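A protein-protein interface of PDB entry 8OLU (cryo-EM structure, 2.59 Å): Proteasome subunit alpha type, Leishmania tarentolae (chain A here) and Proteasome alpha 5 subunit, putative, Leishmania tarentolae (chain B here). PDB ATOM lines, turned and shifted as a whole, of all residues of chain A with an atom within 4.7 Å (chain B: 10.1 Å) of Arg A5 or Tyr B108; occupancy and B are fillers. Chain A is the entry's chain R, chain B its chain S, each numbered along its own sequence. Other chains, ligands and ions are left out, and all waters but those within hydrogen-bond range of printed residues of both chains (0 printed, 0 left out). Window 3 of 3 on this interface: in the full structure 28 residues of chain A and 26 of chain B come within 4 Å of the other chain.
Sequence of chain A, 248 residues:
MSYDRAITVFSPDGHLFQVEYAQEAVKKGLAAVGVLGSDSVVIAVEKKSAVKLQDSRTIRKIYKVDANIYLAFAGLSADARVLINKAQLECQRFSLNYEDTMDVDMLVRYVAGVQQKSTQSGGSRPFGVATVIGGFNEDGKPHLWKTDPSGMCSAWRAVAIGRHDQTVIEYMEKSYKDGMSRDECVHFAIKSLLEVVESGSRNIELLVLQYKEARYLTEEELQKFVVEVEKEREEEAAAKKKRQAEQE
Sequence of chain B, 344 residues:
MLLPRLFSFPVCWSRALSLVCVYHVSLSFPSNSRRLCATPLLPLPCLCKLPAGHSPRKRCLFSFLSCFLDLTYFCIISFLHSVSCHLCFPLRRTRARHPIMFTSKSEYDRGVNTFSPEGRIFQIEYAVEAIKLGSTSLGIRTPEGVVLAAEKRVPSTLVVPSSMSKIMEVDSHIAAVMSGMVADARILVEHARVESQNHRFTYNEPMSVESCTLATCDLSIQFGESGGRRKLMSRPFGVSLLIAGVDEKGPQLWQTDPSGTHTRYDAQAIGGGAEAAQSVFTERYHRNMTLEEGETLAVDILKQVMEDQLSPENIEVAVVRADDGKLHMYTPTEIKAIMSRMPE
The backbone carbonyl oxygen of Arg A5 sits at hydrogen-bond distance from the backbone NH of Gly A123, 2.7 Å away.
Arg A5 touches one residue of chain B.
No residue of chain B comes within 4 Å of Asp A4.
Of the printed residues of chain B, Ile A7 touches Tyr B108.
Gly A122 touches just one residue of chain B: Ser B234 (3.7 Å).
Printed residues of chain A within 4 Å of Gln B123: Val A9.
Printed residues of chain A within 4 Å of Ser B234: Ala A6 (3.7 Å), Thr A8 (3.2 Å) and Gly A122 (3.7 Å).
Of the printed residues of chain A, Arg B235 touches Thr A8 (3.7 Å).
Gly B111 touches none of the printed residues of chain A.
Thr B114 touches none of the printed residues of chain A.
The nearest residue of chain B that does not touch Arg A5 is Ser B234 (5.1 Å).
The nearest residue of chain A that does not touch Tyr B108 is Val A9 (4.1 Å).
Tyr B108 touches Arg A5.
CE1 of Tyr B108 touches O of Ala A6, at 3.4 Å.
Ala A6 touches Ser B234 (CB to O, 3.7 Å).
Arg B235 touches Thr A8.
CG1 of Val A9 touches CG1 of Val B112 (3.7 Å).
Val A9 touches Gln B123.
Gln A18 touches Tyr B108.
CB of Ser B234 touches N of Gly A122, at 3.7 Å.
Hydrophobic or aromatic side chains of chain A that line the printed part of chain B: Ala A6, Ile A7 and Val A9.
Of the 16 printed residues of chain B, 5 touch a printed residue of chain A.
Printed residues of chain B that touch a printed residue of chain A: Tyr B108, Val B112, Gln B123, Ser B234 and Arg B235.
Among the printed residues, 10 pairs touch across the chains.
Among the printed residues, no Asp or Glu carboxylate lies within 4 Å of a Lys or Arg side-chain nitrogen of the other chain.
O of Thr A8 is in hydrogen-bond range of OG of Ser B234.
The side-chain hydroxyl (OH) of Tyr B108 is in hydrogen-bond range of the backbone carbonyl oxygen (O) of Ile A7 (2.4 Å).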
ATOM      1  N   TYR A   3      -1.721 -14.446 -24.883  1.00  0.00           N
ATOM      2  CA  TYR A   3      -1.903 -13.597 -23.721  1.00  0.00           C
ATOM      3  C   TYR A   3      -0.587 -12.912 -23.424  1.00  0.00           C
ATOM      4  O   TYR A   3       0.417 -13.607 -23.264  1.00  0.00           O
ATOM      5  CB  TYR A   3      -2.265 -14.406 -22.502  1.00  0.00           C
ATOM      6  CG  TYR A   3      -2.473 -13.641 -21.222  1.00  0.00           C
ATOM      7  CD1 TYR A   3      -3.624 -12.928 -20.974  1.00  0.00           C
ATOM      8  CD2 TYR A   3      -1.569 -13.723 -20.194  1.00  0.00           C
ATOM      9  CE1 TYR A   3      -3.866 -12.318 -19.747  1.00  0.00           C
ATOM     10  CE2 TYR A   3      -1.783 -13.083 -18.981  1.00  0.00           C
ATOM     11  CZ  TYR A   3      -2.950 -12.411 -18.736  1.00  0.00           C
ATOM     12  OH  TYR A   3      -3.108 -11.774 -17.534  1.00  0.00           O
ATOM     13  N   ASP A   4      -0.631 -11.572 -23.405  1.00  0.00           N
ATOM     14  CA  ASP A   4       0.561 -10.759 -23.282  1.00  0.00           C
ATOM     15  C   ASP A   4       0.273  -9.606 -22.370  1.00  0.00           C
ATOM     16  O   ASP A   4       0.973  -8.632 -22.447  1.00  0.00           O
ATOM     17  CB  ASP A   4       1.087 -10.181 -24.611  1.00  0.00           C
ATOM     18  CG  ASP A   4       0.105  -9.362 -25.466  1.00  0.00           C
ATOM     19  OD1 ASP A   4      -0.388  -8.301 -24.981  1.00  0.00           O
ATOM     20  OD2 ASP A   4      -0.149  -9.762 -26.651  1.00  0.00           O
ATOM     21  N   ARG A   5      -0.662  -9.736 -21.448  1.00  0.00           N
ATOM     22  CA  ARG A   5      -0.800  -8.670 -20.479  1.00  0.00           C
ATOM     23  C   ARG A   5       0.516  -8.452 -19.750  1.00  0.00           C
ATOM     24  O   ARG A   5       1.350  -9.348 -19.640  1.00  0.00           O
ATOM     25  CB  ARG A   5      -1.843  -8.946 -19.406  1.00  0.00           C
ATOM     26  CG  ARG A   5      -2.426  -7.666 -18.820  1.00  0.00           C
ATOM     27  CD  ARG A   5      -3.378  -8.049 -17.708  1.00  0.00           C
ATOM     28  NE  ARG A   5      -4.085  -6.924 -17.117  1.00  0.00           N
ATOM     29  CZ  ARG A   5      -4.236  -6.775 -15.811  1.00  0.00           C
ATOM     30  NH1 ARG A   5      -3.271  -7.173 -14.998  1.00  0.00           N
ATOM     31  NH2 ARG A   5      -5.348  -6.251 -15.326  1.00  0.00           N
ATOM     32  N   ALA A   6       0.666  -7.243 -19.233  1.00  0.00           N
ATOM     33  CA  ALA A   6       1.852  -6.850 -18.516  1.00  0.00           C
ATOM     34  C   ALA A   6       1.662  -7.190 -17.053  1.00  0.00           C
ATOM     35  O   ALA A   6       0.958  -6.458 -16.364  1.00  0.00           O
ATOM     36  CB  ALA A   6       2.098  -5.361 -18.694  1.00  0.00           C
ATOM     37  N   ILE A   7       2.405  -8.205 -16.596  1.00  0.00           N
ATOM     38  CA  ILE A   7       2.279  -8.738 -15.253  1.00  0.00           C
ATOM     39  C   ILE A   7       3.221  -8.008 -14.300  1.00  0.00           C
ATOM     40  O   ILE A   7       2.824  -7.518 -13.256  1.00  0.00           O
ATOM     41  CB  ILE A   7       2.526 -10.247 -15.306  1.00  0.00           C
ATOM     42  CG1 ILE A   7       1.317 -10.949 -15.928  1.00  0.00           C
ATOM     43  CG2 ILE A   7       2.829 -10.804 -13.939  1.00  0.00           C
ATOM     44  CD1 ILE A   7       1.605 -12.365 -16.409  1.00  0.00           C
ATOM     45  N   THR A   8       4.456  -7.869 -14.724  1.00  0.00           N
ATOM     46  CA  THR A   8       5.464  -7.179 -13.963  1.00  0.00           C
ATOM     47  C   THR A   8       5.459  -5.714 -14.384  1.00  0.00           C
ATOM     48  O   THR A   8       5.821  -5.400 -15.516  1.00  0.00           O
ATOM     49  CB  THR A   8       6.833  -7.842 -14.196  1.00  0.00           C
ATOM     50  OG1 THR A   8       6.763  -9.273 -14.115  1.00  0.00           O
ATOM     51  CG2 THR A   8       7.870  -7.350 -13.201  1.00  0.00           C
ATOM     52  N   VAL A   9       5.107  -4.827 -13.454  1.00  0.00           N
ATOM     53  CA  VAL A   9       5.032  -3.407 -13.753  1.00  0.00           C
ATOM     54  C   VAL A   9       5.522  -2.613 -12.566  1.00  0.00           C
ATOM     55  O   VAL A   9       5.434  -3.073 -11.436  1.00  0.00           O
ATOM     56  CB  VAL A   9       3.575  -3.012 -14.039  1.00  0.00           C
ATOM     57  CG1 VAL A   9       3.062  -3.739 -15.251  1.00  0.00           C
ATOM     58  CG2 VAL A   9       2.650  -3.316 -12.885  1.00  0.00           C
ATOM     59  N   GLN A  18       5.953  -7.811  -8.608  1.00  0.00           N
ATOM     60  CA  GLN A  18       6.068  -9.207  -8.943  1.00  0.00           C
ATOM     61  C   GLN A  18       7.467  -9.751  -8.714  1.00  0.00           C
ATOM     62  O   GLN A  18       7.633 -10.959  -8.598  1.00  0.00           O
ATOM     63  CB  GLN A  18       5.774  -9.458 -10.419  1.00  0.00           C
ATOM     64  CG  GLN A  18       4.273  -9.423 -10.741  1.00  0.00           C
ATOM     65  CD  GLN A  18       3.575 -10.404  -9.866  1.00  0.00           C
ATOM     66  OE1 GLN A  18       3.699 -11.592 -10.123  1.00  0.00           O
ATOM     67  NE2 GLN A  18       2.943  -9.913  -8.805  1.00  0.00           N
ATOM     68  N   GLY A 122       5.548  -9.753 -21.292  1.00  0.00           N
ATOM     69  CA  GLY A 122       4.127  -9.738 -21.052  1.00  0.00           C
ATOM     70  C   GLY A 122       3.626 -11.165 -21.180  1.00  0.00           C
ATOM     71  O   GLY A 122       3.982 -11.871 -22.121  1.00  0.00           O
ATOM     72  N   GLY A 123       2.802 -11.530 -20.199  1.00  0.00           N
ATOM     73  CA  GLY A 123       2.103 -12.787 -20.223  1.00  0.00           C
ATOM     74  C   GLY A 123       2.631 -13.713 -19.144  1.00  0.00           C
ATOM     75  O   GLY A 123       1.954 -14.682 -18.767  1.00  0.00           O
ATOM     76  N   GLU B 107      -2.834  -1.852  -8.502  1.00  0.00           N
ATOM     77  CA  GLU B 107      -1.640  -1.452  -9.308  1.00  0.00           C
ATOM     78  C   GLU B 107      -1.779  -1.868 -10.781  1.00  0.00           C
ATOM     79  O   GLU B 107      -0.991  -1.437 -11.626  1.00  0.00           O
ATOM     80  CB  GLU B 107      -0.330  -1.981  -8.695  1.00  0.00           C
ATOM     81  CG  GLU B 107       0.128  -3.379  -9.147  1.00  0.00           C
ATOM     82  CD  GLU B 107       0.179  -4.469  -8.082  1.00  0.00           C
ATOM     83  OE1 GLU B 107      -0.205  -4.190  -6.925  1.00  0.00           O
ATOM     84  OE2 GLU B 107       0.617  -5.602  -8.405  1.00  0.00           O
ATOM     85  N   TYR B 108      -2.765  -2.725 -11.083  1.00  0.00           N
ATOM     86  CA  TYR B 108      -3.163  -3.053 -12.446  1.00  0.00           C
ATOM     87  C   TYR B 108      -4.431  -2.267 -12.812  1.00  0.00           C
ATOM     88  O   TYR B 108      -5.070  -2.534 -13.828  1.00  0.00           O
ATOM     89  CB  TYR B 108      -3.404  -4.565 -12.574  1.00  0.00           C
ATOM     90  CG  TYR B 108      -2.215  -5.483 -12.360  1.00  0.00           C
ATOM     91  CD1 TYR B 108      -1.165  -5.546 -13.275  1.00  0.00           C
ATOM     92  CD2 TYR B 108      -2.159  -6.343 -11.267  1.00  0.00           C
ATOM     93  CE1 TYR B 108      -0.085  -6.401 -13.092  1.00  0.00           C
ATOM     94  CE2 TYR B 108      -1.089  -7.207 -11.071  1.00  0.00           C
ATOM     95  CZ  TYR B 108      -0.045  -7.238 -11.985  1.00  0.00           C
ATOM     96  OH  TYR B 108       1.014  -8.094 -11.786  1.00  0.00           O
ATOM     97  N   ASP B 109      -4.786  -1.296 -11.960  1.00  0.00           N
ATOM     98  CA  ASP B 109      -5.960  -0.456 -12.132  1.00  0.00           C
ATOM     99  C   ASP B 109      -5.765   0.329 -13.440  1.00  0.00           C
ATOM    100  O   ASP B 109      -6.593   0.281 -14.349  1.00  0.00           O
ATOM    101  CB  ASP B 109      -6.143   0.379 -10.843  1.00  0.00           C
ATOM    102  CG  ASP B 109      -7.547   0.453 -10.245  1.00  0.00           C
ATOM    103  OD1 ASP B 109      -8.279  -0.556 -10.325  1.00  0.00           O
ATOM    104  OD2 ASP B 109      -7.883   1.506  -9.649  1.00  0.00           O
ATOM    105  N   ARG B 110      -4.617   1.017 -13.528  1.00  0.00           N
ATOM    106  CA  ARG B 110      -4.180   1.758 -14.700  1.00  0.00           C
ATOM    107  C   ARG B 110      -3.241   0.897 -15.535  1.00  0.00           C
ATOM    108  O   ARG B 110      -2.160   0.543 -15.061  1.00  0.00           O
ATOM    109  CB  ARG B 110      -3.376   2.993 -14.275  1.00  0.00           C
ATOM    110  CG  ARG B 110      -4.206   4.059 -13.575  1.00  0.00           C
ATOM    111  CD  ARG B 110      -3.370   5.249 -13.179  1.00  0.00           C
ATOM    112  NE  ARG B 110      -2.815   5.229 -11.831  1.00  0.00           N
ATOM    113  CZ  ARG B 110      -3.019   6.187 -10.927  1.00  0.00           C
ATOM    114  NH1 ARG B 110      -2.341   6.194  -9.792  1.00  0.00           N
ATOM    115  NH2 ARG B 110      -3.898   7.150 -11.164  1.00  0.00           N
ATOM    116  N   GLY B 111      -3.647   0.592 -16.774  1.00  0.00           N
ATOM    117  CA  GLY B 111      -2.752   0.052 -17.791  1.00  0.00           C
ATOM    118  C   GLY B 111      -1.477   0.885 -17.942  1.00  0.00           C
ATOM    119  O   GLY B 111      -1.370   1.981 -17.392  1.00  0.00           O
ATOM    120  N   VAL B 112      -0.521   0.364 -18.712  1.00  0.00           N
ATOM    121  CA  VAL B 112       0.868   0.791 -18.608  1.00  0.00           C
ATOM    122  C   VAL B 112       1.219   1.920 -19.584  1.00  0.00           C
ATOM    123  O   VAL B 112       2.285   2.545 -19.510  1.00  0.00           O
ATOM    124  CB  VAL B 112       1.774  -0.422 -18.857  1.00  0.00           C
ATOM    125  CG1 VAL B 112       1.551  -1.477 -17.779  1.00  0.00           C
ATOM    126  CG2 VAL B 112       1.607  -0.984 -20.269  1.00  0.00           C
ATOM    127  N   ASN B 113       0.292   2.134 -20.516  1.00  0.00           N
ATOM    128  CA  ASN B 113       0.384   3.145 -21.537  1.00  0.00           C
ATOM    129  C   ASN B 113      -0.467   4.345 -21.147  1.00  0.00           C
ATOM    130  O   ASN B 113      -0.925   5.092 -21.974  1.00  0.00           O
ATOM    131  CB  ASN B 113      -0.156   2.544 -22.836  1.00  0.00           C
ATOM    132  CG  ASN B 113       0.917   2.043 -23.774  1.00  0.00           C
ATOM    133  OD1 ASN B 113       2.117   2.184 -23.508  1.00  0.00           O
ATOM    134  ND2 ASN B 113       0.453   1.483 -24.882  1.00  0.00           N
ATOM    135  N   THR B 114      -0.697   4.540 -19.880  1.00  0.00           N
ATOM    136  CA  THR B 114      -1.679   5.508 -19.480  1.00  0.00           C
ATOM    137  C   THR B 114      -1.008   6.821 -19.129  1.00  0.00           C
ATOM    138  O   THR B 114       0.017   6.791 -18.462  1.00  0.00           O
ATOM    139  CB  THR B 114      -2.424   4.972 -18.265  1.00  0.00           C
ATOM    140  OG1 THR B 114      -3.140   3.874 -18.825  1.00  0.00           O
ATOM    141  CG2 THR B 114      -3.290   6.028 -17.614  1.00  0.00           C
ATOM    142  N   GLN B 123       3.994   4.602 -15.798  1.00  0.00           N
ATOM    143  CA  GLN B 123       5.058   3.652 -15.639  1.00  0.00           C
ATOM    144  C   GLN B 123       6.400   4.335 -15.869  1.00  0.00           C
ATOM    145  O   GLN B 123       7.389   3.866 -15.321  1.00  0.00           O
ATOM    146  CB  GLN B 123       4.925   2.473 -16.605  1.00  0.00           C
ATOM    147  CG  GLN B 123       3.819   1.503 -16.221  1.00  0.00           C
ATOM    148  CD  GLN B 123       4.035   0.892 -14.864  1.00  0.00           C
ATOM    149  OE1 GLN B 123       4.846  -0.018 -14.707  1.00  0.00           O
ATOM    150  NE2 GLN B 123       3.338   1.430 -13.882  1.00  0.00           N
ATOM    151  N   TYR B 126       7.335   6.106 -12.573  1.00  0.00           N
ATOM    152  CA  TYR B 126       7.697   5.092 -11.614  1.00  0.00           C
ATOM    153  C   TYR B 126       9.043   4.501 -12.004  1.00  0.00           C
ATOM    154  O   TYR B 126       9.942   4.428 -11.218  1.00  0.00           O
ATOM    155  CB  TYR B 126       6.604   4.024 -11.545  1.00  0.00           C
ATOM    156  CG  TYR B 126       5.198   4.465 -11.205  1.00  0.00           C
ATOM    157  CD1 TYR B 126       4.903   5.678 -10.576  1.00  0.00           C
ATOM    158  CD2 TYR B 126       4.128   3.642 -11.542  1.00  0.00           C
ATOM    159  CE1 TYR B 126       3.585   6.044 -10.304  1.00  0.00           C
ATOM    160  CE2 TYR B 126       2.806   4.019 -11.308  1.00  0.00           C
ATOM    161  CZ  TYR B 126       2.533   5.226 -10.697  1.00  0.00           C
ATOM    162  OH  TYR B 126       1.202   5.513 -10.476  1.00  0.00           O
ATOM    163  N   PHE B 223       7.421  -0.646 -25.216  1.00  0.00           N
ATOM    164  CA  PHE B 223       6.700  -1.225 -24.082  1.00  0.00           C
ATOM    165  C   PHE B 223       5.175  -1.003 -24.203  1.00  0.00           C
ATOM    166  O   PHE B 223       4.706   0.072 -24.598  1.00  0.00           O
ATOM    167  CB  PHE B 223       7.348  -0.787 -22.748  1.00  0.00           C
ATOM    168  CG  PHE B 223       7.158   0.648 -22.311  1.00  0.00           C
ATOM    169  CD1 PHE B 223       6.037   1.018 -21.563  1.00  0.00           C
ATOM    170  CD2 PHE B 223       8.102   1.621 -22.636  1.00  0.00           C
ATOM    171  CE1 PHE B 223       5.841   2.338 -21.187  1.00  0.00           C
ATOM    172  CE2 PHE B 223       7.898   2.944 -22.268  1.00  0.00           C
ATOM    173  CZ  PHE B 223       6.767   3.298 -21.548  1.00  0.00           C
ATOM    174  N   GLY B 224       4.410  -2.065 -23.859  1.00  0.00           N
ATOM    175  CA  GLY B 224       2.957  -2.130 -23.979  1.00  0.00           C
ATOM    176  C   GLY B 224       2.399  -3.412 -23.369  1.00  0.00           C
ATOM    177  O   GLY B 224       1.431  -3.963 -23.946  1.00  0.00           O
ATOM    178  N   LEU B 232       5.672  -7.141 -27.069  1.00  0.00           N
ATOM    179  CA  LEU B 232       6.822  -6.255 -26.733  1.00  0.00           C
ATOM    180  C   LEU B 232       7.027  -6.232 -25.208  1.00  0.00           C
ATOM    181  O   LEU B 232       6.455  -7.061 -24.496  1.00  0.00           O
ATOM    182  CB  LEU B 232       6.584  -4.875 -27.378  1.00  0.00           C
ATOM    183  CG  LEU B 232       7.078  -4.710 -28.829  1.00  0.00           C
ATOM    184  CD1 LEU B 232       8.496  -5.271 -29.030  1.00  0.00           C
ATOM    185  CD2 LEU B 232       6.120  -5.334 -29.846  1.00  0.00           C
ATOM    186  N   MET B 233       7.902  -5.338 -24.711  1.00  0.00           N
ATOM    187  CA  MET B 233       8.324  -5.346 -23.315  1.00  0.00           C
ATOM    188  C   MET B 233       7.150  -4.935 -22.414  1.00  0.00           C
ATOM    189  O   MET B 233       6.552  -3.878 -22.558  1.00  0.00           O
ATOM    190  CB  MET B 233       9.497  -4.384 -23.027  1.00  0.00           C
ATOM    191  CG  MET B 233      10.771  -4.566 -23.860  1.00  0.00           C
ATOM    192  SD  MET B 233      11.797  -6.009 -23.416  1.00  0.00           S
ATOM    193  CE  MET B 233      13.291  -5.674 -24.362  1.00  0.00           C
ATOM    194  N   SER B 234       6.865  -5.760 -21.419  1.00  0.00           N
ATOM    195  CA  SER B 234       5.800  -5.468 -20.489  1.00  0.00           C
ATOM    196  C   SER B 234       5.915  -4.039 -19.968  1.00  0.00           C
ATOM    197  O   SER B 234       4.935  -3.333 -20.037  1.00  0.00           O
ATOM    198  CB  SER B 234       5.658  -6.569 -19.369  1.00  0.00           C
ATOM    199  OG  SER B 234       6.650  -6.565 -18.332  1.00  0.00           O
ATOM    200  N   ARG B 235       7.103  -3.597 -19.557  1.00  0.00           N
ATOM    201  CA  ARG B 235       7.293  -2.376 -18.774  1.00  0.00           C
ATOM    202  C   ARG B 235       8.545  -1.671 -19.256  1.00  0.00           C
ATOM    203  O   ARG B 235       9.341  -2.275 -19.947  1.00  0.00           O
ATOM    204  CB  ARG B 235       7.605  -2.664 -17.302  1.00  0.00           C
ATOM    205  CG  ARG B 235       8.672  -3.741 -17.132  1.00  0.00           C
ATOM    206  CD  ARG B 235       9.199  -3.846 -15.724  1.00  0.00           C
ATOM    207  NE  ARG B 235      10.203  -4.904 -15.690  1.00  0.00           N
ATOM    208  CZ  ARG B 235      11.506  -4.679 -15.686  1.00  0.00           C
ATOM    209  NH1 ARG B 235      11.994  -3.437 -15.745  1.00  0.00           N
ATOM    210  NH2 ARG B 235      12.291  -5.726 -15.633  1.00  0.00           N
